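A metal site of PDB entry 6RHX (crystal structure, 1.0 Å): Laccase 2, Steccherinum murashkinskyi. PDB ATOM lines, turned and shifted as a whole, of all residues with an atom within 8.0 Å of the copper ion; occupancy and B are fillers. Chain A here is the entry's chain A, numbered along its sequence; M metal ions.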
ATOM      1  N   CYS A 208     -19.838  15.138 -15.798  1.00  0.00           N
ATOM      2  CA  CYS A 208     -19.528  15.203 -14.384  1.00  0.00           C
ATOM      3  C   CYS A 208     -18.970  13.916 -13.823  1.00  0.00           C
ATOM      4  O   CYS A 208     -18.476  13.925 -12.677  1.00  0.00           O
ATOM      5  CB  CYS A 208     -20.729  15.582 -13.545  1.00  0.00           C
ATOM      6  SG  CYS A 208     -20.813  17.381 -13.293  1.00  0.00           S
ATOM      7  N   ASP A 209     -19.043  12.795 -14.558  1.00  0.00           N
ATOM      8  CA  ASP A 209     -18.628  11.506 -13.972  1.00  0.00           C
ATOM      9  C   ASP A 209     -18.317  10.479 -15.036  1.00  0.00           C
ATOM     10  O   ASP A 209     -17.149  10.171 -15.230  1.00  0.00           O
ATOM     11  CB  ASP A 209     -19.634  11.068 -12.909  1.00  0.00           C
ATOM     12  CG  ASP A 209     -19.394   9.694 -12.359  1.00  0.00           C
ATOM     13  OD1 ASP A 209     -18.531   8.966 -12.776  1.00  0.00           O
ATOM     14  OD2 ASP A 209     -20.278   9.267 -11.531  1.00  0.00           O
ATOM     15  N   PHE A 341     -11.995  11.510  -0.407  1.00  0.00           N
ATOM     16  CA  PHE A 341     -10.734  11.303  -1.092  1.00  0.00           C
ATOM     17  C   PHE A 341      -9.638  12.097  -0.405  1.00  0.00           C
ATOM     18  O   PHE A 341      -9.863  13.111   0.257  1.00  0.00           O
ATOM     19  CB  PHE A 341     -10.857  11.758  -2.541  1.00  0.00           C
ATOM     20  CG  PHE A 341     -11.690  10.852  -3.369  1.00  0.00           C
ATOM     21  CD1 PHE A 341     -13.052  11.064  -3.561  1.00  0.00           C
ATOM     22  CD2 PHE A 341     -11.110   9.738  -3.992  1.00  0.00           C
ATOM     23  CE1 PHE A 341     -13.807  10.215  -4.311  1.00  0.00           C
ATOM     24  CE2 PHE A 341     -11.885   8.898  -4.771  1.00  0.00           C
ATOM     25  CZ  PHE A 341     -13.236   9.122  -4.914  1.00  0.00           C
ATOM     26  N   ALA A 392      -7.572   3.883  -5.814  1.00  0.00           N
ATOM     27  CA  ALA A 392      -8.660   4.518  -5.025  1.00  0.00           C
ATOM     28  C   ALA A 392      -9.999   4.137  -5.633  1.00  0.00           C
ATOM     29  O   ALA A 392     -10.138   4.192  -6.862  1.00  0.00           O
ATOM     30  CB  ALA A 392      -8.493   6.045  -5.003  1.00  0.00           C
ATOM     31  N   ALA A 393     -11.004   3.872  -4.783  1.00  0.00           N
ATOM     32  CA  ALA A 393     -12.340   3.535  -5.233  1.00  0.00           C
ATOM     33  C   ALA A 393     -12.899   4.596  -6.151  1.00  0.00           C
ATOM     34  O   ALA A 393     -12.509   5.782  -6.120  1.00  0.00           O
ATOM     35  CB  ALA A 393     -13.224   3.386  -4.011  1.00  0.00           C
ATOM     36  N   GLY A 394     -13.849   4.156  -6.978  1.00  0.00           N
ATOM     37  CA  GLY A 394     -14.541   5.043  -7.871  1.00  0.00           C
ATOM     38  C   GLY A 394     -13.864   5.287  -9.178  1.00  0.00           C
ATOM     39  O   GLY A 394     -14.272   6.172  -9.899  1.00  0.00           O
ATOM     40  N   GLY A 395     -12.818   4.517  -9.481  1.00  0.00           N
ATOM     41  CA  GLY A 395     -12.058   4.718 -10.724  1.00  0.00           C
ATOM     42  C   GLY A 395     -12.842   4.205 -11.937  1.00  0.00           C
ATOM     43  O   GLY A 395     -13.890   3.573 -11.813  1.00  0.00           O
ATOM     44  N   PRO A 396     -12.303   4.444 -13.129  1.00  0.00           N
ATOM     45  CA  PRO A 396     -11.004   5.092 -13.380  1.00  0.00           C
ATOM     46  C   PRO A 396     -11.116   6.601 -13.287  1.00  0.00           C
ATOM     47  O   PRO A 396     -12.032   7.233 -13.846  1.00  0.00           O
ATOM     48  CB  PRO A 396     -10.663   4.631 -14.787  1.00  0.00           C
ATOM     49  CG  PRO A 396     -11.996   4.394 -15.446  1.00  0.00           C
ATOM     50  CD  PRO A 396     -12.867   3.887 -14.352  1.00  0.00           C
ATOM     51  N   HIS A 397     -10.173   7.209 -12.571  1.00  0.00           N
ATOM     52  CA  HIS A 397     -10.213   8.627 -12.288  1.00  0.00           C
ATOM     53  C   HIS A 397      -9.516   9.437 -13.364  1.00  0.00           C
ATOM     54  O   HIS A 397      -8.314   9.221 -13.588  1.00  0.00           O
ATOM     55  CB  HIS A 397      -9.531   8.926 -10.929  1.00  0.00           C
ATOM     56  CG  HIS A 397     -10.143   8.189  -9.808  1.00  0.00           C
ATOM     57  ND1 HIS A 397     -11.339   8.601  -9.234  1.00  0.00           N
ATOM     58  CD2 HIS A 397      -9.695   7.108  -9.118  1.00  0.00           C
ATOM     59  CE1 HIS A 397     -11.612   7.723  -8.280  1.00  0.00           C
ATOM     60  NE2 HIS A 397     -10.649   6.822  -8.181  1.00  0.00           N
ATOM     61  N   PRO A 398     -10.201  10.401 -13.990  1.00  0.00           N
ATOM     62  CA  PRO A 398      -9.574  11.279 -14.971  1.00  0.00           C
ATOM     63  C   PRO A 398      -8.972  12.511 -14.311  1.00  0.00           C
ATOM     64  O   PRO A 398      -9.671  13.469 -13.988  1.00  0.00           O
ATOM     65  CB  PRO A 398     -10.705  11.613 -15.931  1.00  0.00           C
ATOM     66  CG  PRO A 398     -11.940  11.632 -15.015  1.00  0.00           C
ATOM     67  CD  PRO A 398     -11.660  10.586 -13.957  1.00  0.00           C
ATOM     68  N   PHE A 399      -7.666  12.489 -14.106  1.00  0.00           N
ATOM     69  CA  PHE A 399      -6.975  13.602 -13.467  1.00  0.00           C
ATOM     70  C   PHE A 399      -6.666  14.690 -14.459  1.00  0.00           C
ATOM     71  O   PHE A 399      -6.239  14.450 -15.587  1.00  0.00           O
ATOM     72  CB  PHE A 399      -5.701  13.125 -12.735  1.00  0.00           C
ATOM     73  CG  PHE A 399      -5.950  12.831 -11.298  1.00  0.00           C
ATOM     74  CD1 PHE A 399      -6.683  11.716 -10.904  1.00  0.00           C
ATOM     75  CD2 PHE A 399      -5.540  13.728 -10.302  1.00  0.00           C
ATOM     76  CE1 PHE A 399      -7.004  11.525  -9.567  1.00  0.00           C
ATOM     77  CE2 PHE A 399      -5.863  13.515  -8.964  1.00  0.00           C
ATOM     78  CZ  PHE A 399      -6.580  12.410  -8.603  1.00  0.00           C
ATOM     79  N   ILE A 430      -6.202   7.678 -14.940  1.00  0.00           N
ATOM     80  CA  ILE A 430      -5.129   7.031 -14.195  1.00  0.00           C
ATOM     81  C   ILE A 430      -5.290   5.524 -14.128  1.00  0.00           C
ATOM     82  O   ILE A 430      -4.447   4.817 -13.587  1.00  0.00           O
ATOM     83  CB  ILE A 430      -4.839   7.669 -12.857  1.00  0.00           C
ATOM     84  CG1 ILE A 430      -5.942   7.402 -11.855  1.00  0.00           C
ATOM     85  CG2 ILE A 430      -4.574   9.181 -13.016  1.00  0.00           C
ATOM     86  CD1 ILE A 430      -5.600   7.816 -10.438  1.00  0.00           C
ATOM     87  N   HIS A 452      -6.747  17.842 -10.014  1.00  0.00           N
ATOM     88  CA  HIS A 452      -7.848  17.132  -9.386  1.00  0.00           C
ATOM     89  C   HIS A 452      -8.423  16.099 -10.304  1.00  0.00           C
ATOM     90  O   HIS A 452      -8.302  16.170 -11.521  1.00  0.00           O
ATOM     91  CB  HIS A 452      -8.933  18.124  -8.933  1.00  0.00           C
ATOM     92  CG  HIS A 452      -9.589  18.901 -10.033  1.00  0.00           C
ATOM     93  ND1 HIS A 452     -10.670  18.430 -10.733  1.00  0.00           N
ATOM     94  CD2 HIS A 452      -9.322  20.116 -10.536  1.00  0.00           C
ATOM     95  CE1 HIS A 452     -11.018  19.351 -11.614  1.00  0.00           C
ATOM     96  NE2 HIS A 452     -10.221  20.407 -11.527  1.00  0.00           N
ATOM     97  N   CYS A 453      -9.148  15.141  -9.679  1.00  0.00           N
ATOM     98  CA  CYS A 453      -9.989  14.255 -10.479  1.00  0.00           C
ATOM     99  C   CYS A 453     -11.154  15.076 -11.064  1.00  0.00           C
ATOM    100  O   CYS A 453     -11.741  15.873 -10.349  1.00  0.00           O
ATOM    101  CB  CYS A 453     -10.562  13.154  -9.579  1.00  0.00           C
ATOM    102  SG  CYS A 453     -11.558  12.029 -10.597  1.00  0.00           S
ATOM    103  N   HIS A 454     -11.451  14.868 -12.329  1.00  0.00           N
ATOM    104  CA  HIS A 454     -12.518  15.591 -13.009  1.00  0.00           C
ATOM    105  C   HIS A 454     -13.866  14.920 -12.902  1.00  0.00           C
ATOM    106  O   HIS A 454     -14.839  15.444 -13.468  1.00  0.00           O
ATOM    107  CB  HIS A 454     -12.144  15.914 -14.441  1.00  0.00           C
ATOM    108  CG  HIS A 454     -12.622  17.259 -14.903  1.00  0.00           C
ATOM    109  ND1 HIS A 454     -13.944  17.631 -14.958  1.00  0.00           N
ATOM    110  CD2 HIS A 454     -11.949  18.375 -15.300  1.00  0.00           C
ATOM    111  CE1 HIS A 454     -14.014  18.904 -15.368  1.00  0.00           C
ATOM    112  NE2 HIS A 454     -12.816  19.392 -15.598  1.00  0.00           N
ATOM    113  N   ILE A 455     -13.984  13.836 -12.132  1.00  0.00           N
ATOM    114  CA  ILE A 455     -15.311  13.371 -11.718  1.00  0.00           C
ATOM    115  C   ILE A 455     -15.723  14.347 -10.620  1.00  0.00           C
ATOM    116  O   ILE A 455     -15.107  14.423  -9.552  1.00  0.00           O
ATOM    117  CB  ILE A 455     -15.267  11.920 -11.243  1.00  0.00           C
ATOM    118  CG1 ILE A 455     -14.919  11.000 -12.408  1.00  0.00           C
ATOM    119  CG2 ILE A 455     -16.607  11.542 -10.592  1.00  0.00           C
ATOM    120  CD1 ILE A 455     -14.557   9.574 -12.030  1.00  0.00           C
ATOM    121  N   ASP A 456     -16.737  15.171 -10.909  1.00  0.00           N
ATOM    122  CA  ASP A 456     -16.984  16.319 -10.062  1.00  0.00           C
ATOM    123  C   ASP A 456     -17.397  15.922  -8.662  1.00  0.00           C
ATOM    124  O   ASP A 456     -17.104  16.617  -7.681  1.00  0.00           O
ATOM    125  CB  ASP A 456     -18.021  17.238 -10.738  1.00  0.00           C
ATOM    126  CG  ASP A 456     -17.833  18.715 -10.453  1.00  0.00           C
ATOM    127  OD1 ASP A 456     -16.658  19.111 -10.323  1.00  0.00           O
ATOM    128  OD2 ASP A 456     -18.843  19.438 -10.414  1.00  0.00           O
ATOM    129  N   TRP A 457     -18.065  14.766  -8.534  1.00  0.00           N
ATOM    130  CA  TRP A 457     -18.440  14.272  -7.232  1.00  0.00           C
ATOM    131  C   TRP A 457     -17.210  13.934  -6.373  1.00  0.00           C
ATOM    132  O   TRP A 457     -17.234  14.016  -5.156  1.00  0.00           O
ATOM    133  CB  TRP A 457     -19.360  13.011  -7.383  1.00  0.00           C
ATOM    134  CG  TRP A 457     -20.447  13.215  -8.399  1.00  0.00           C
ATOM    135  CD1 TRP A 457     -20.581  12.567  -9.612  1.00  0.00           C
ATOM    136  CD2 TRP A 457     -21.542  14.115  -8.322  1.00  0.00           C
ATOM    137  NE1 TRP A 457     -21.662  13.026 -10.283  1.00  0.00           N
ATOM    138  CE2 TRP A 457     -22.294  13.988  -9.524  1.00  0.00           C
ATOM    139  CE3 TRP A 457     -22.004  15.009  -7.365  1.00  0.00           C
ATOM    140  CZ2 TRP A 457     -23.430  14.728  -9.774  1.00  0.00           C
ATOM    141  CZ3 TRP A 457     -23.102  15.735  -7.629  1.00  0.00           C
ATOM    142  CH2 TRP A 457     -23.814  15.596  -8.823  1.00  0.00           C
ATOM    143  N   HIS A 458     -16.131  13.534  -7.046  1.00  0.00           N
ATOM    144  CA  HIS A 458     -14.880  13.209  -6.351  1.00  0.00           C
ATOM    145  C   HIS A 458     -14.106  14.461  -5.972  1.00  0.00           C
ATOM    146  O   HIS A 458     -13.524  14.501  -4.888  1.00  0.00           O
ATOM    147  CB  HIS A 458     -14.017  12.286  -7.238  1.00  0.00           C
ATOM    148  CG  HIS A 458     -14.633  10.979  -7.559  1.00  0.00           C
ATOM    149  ND1 HIS A 458     -13.988  10.081  -8.395  1.00  0.00           N
ATOM    150  CD2 HIS A 458     -15.821  10.451  -7.136  1.00  0.00           C
ATOM    151  CE1 HIS A 458     -14.796   9.025  -8.450  1.00  0.00           C
ATOM    152  NE2 HIS A 458     -15.896   9.219  -7.721  1.00  0.00           N
ATOM    153  N   LEU A 459     -14.085  15.459  -6.857  1.00  0.00           N
ATOM    154  CA  LEU A 459     -13.541  16.759  -6.487  1.00  0.00           C
ATOM    155  C   LEU A 459     -14.233  17.300  -5.250  1.00  0.00           C
ATOM    156  O   LEU A 459     -13.581  17.743  -4.291  1.00  0.00           O
ATOM    157  CB  LEU A 459     -13.652  17.708  -7.647  1.00  0.00           C
ATOM    158  CG  LEU A 459     -13.323  19.182  -7.346  1.00  0.00           C
ATOM    159  CD1 LEU A 459     -11.915  19.343  -6.812  1.00  0.00           C
ATOM    160  CD2 LEU A 459     -13.530  20.026  -8.590  1.00  0.00           C
ATOM    161  N   PHE A 463     -10.828  15.226  -3.762  1.00  0.00           N
ATOM    162  CA  PHE A 463      -9.742  14.568  -4.559  1.00  0.00           C
ATOM    163  C   PHE A 463      -8.968  15.625  -5.377  1.00  0.00           C
ATOM    164  O   PHE A 463      -9.087  15.691  -6.598  1.00  0.00           O
ATOM    165  CB  PHE A 463     -10.322  13.486  -5.423  1.00  0.00           C
ATOM    166  CG  PHE A 463      -9.426  12.292  -5.702  1.00  0.00           C
ATOM    167  CD1 PHE A 463      -8.254  12.028  -5.003  1.00  0.00           C
ATOM    168  CD2 PHE A 463      -9.847  11.372  -6.644  1.00  0.00           C
ATOM    169  CE1 PHE A 463      -7.572  10.847  -5.208  1.00  0.00           C
ATOM    170  CE2 PHE A 463      -9.136  10.182  -6.872  1.00  0.00           C
ATOM    171  CZ  PHE A 463      -8.019   9.922  -6.138  1.00  0.00           C
HETATM  172 CU    CU M   1     -12.306  10.363  -9.409  1.00  0.00          CU
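ND1 of His 458 binds the copper ion.
A ring nitrogen (ND1) of His 397 is bound to the copper ion, at 2.0 Å.
SG of Cys 453 is bound to the copper ion.
Ile 455 touches the copper ion (CD1 to CU, 3.5 Å).
Phe 463 touches the copper ion.
O of His 458 lies within hydrogen-bond range of N of Phe 463 (3.0 Å).
O of Ala 393 lies within hydrogen-bond range of NE2 of His 397 (3.0 Å).
A ring nitrogen (NE2) of His 397 lies within hydrogen-bond range of the backbone NH of Gly 395 (3.4 Å).
A ring nitrogen (NE2) of His 397 lies within hydrogen-bond range of the backbone carbonyl oxygen (O) of Ala 392.
The backbone carbonyl oxygen (O) of His 397 sits at hydrogen-bond distance from the backbone NH (N) of Ile 430.
N of Ile 455 lies close to SG of Cys 453, 3.4 Å away.
The backbone carbonyl oxygen (O) of Phe 463 is in hydrogen-bond range of the backbone NH (N) of Cys 453, at 3.1 Å.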
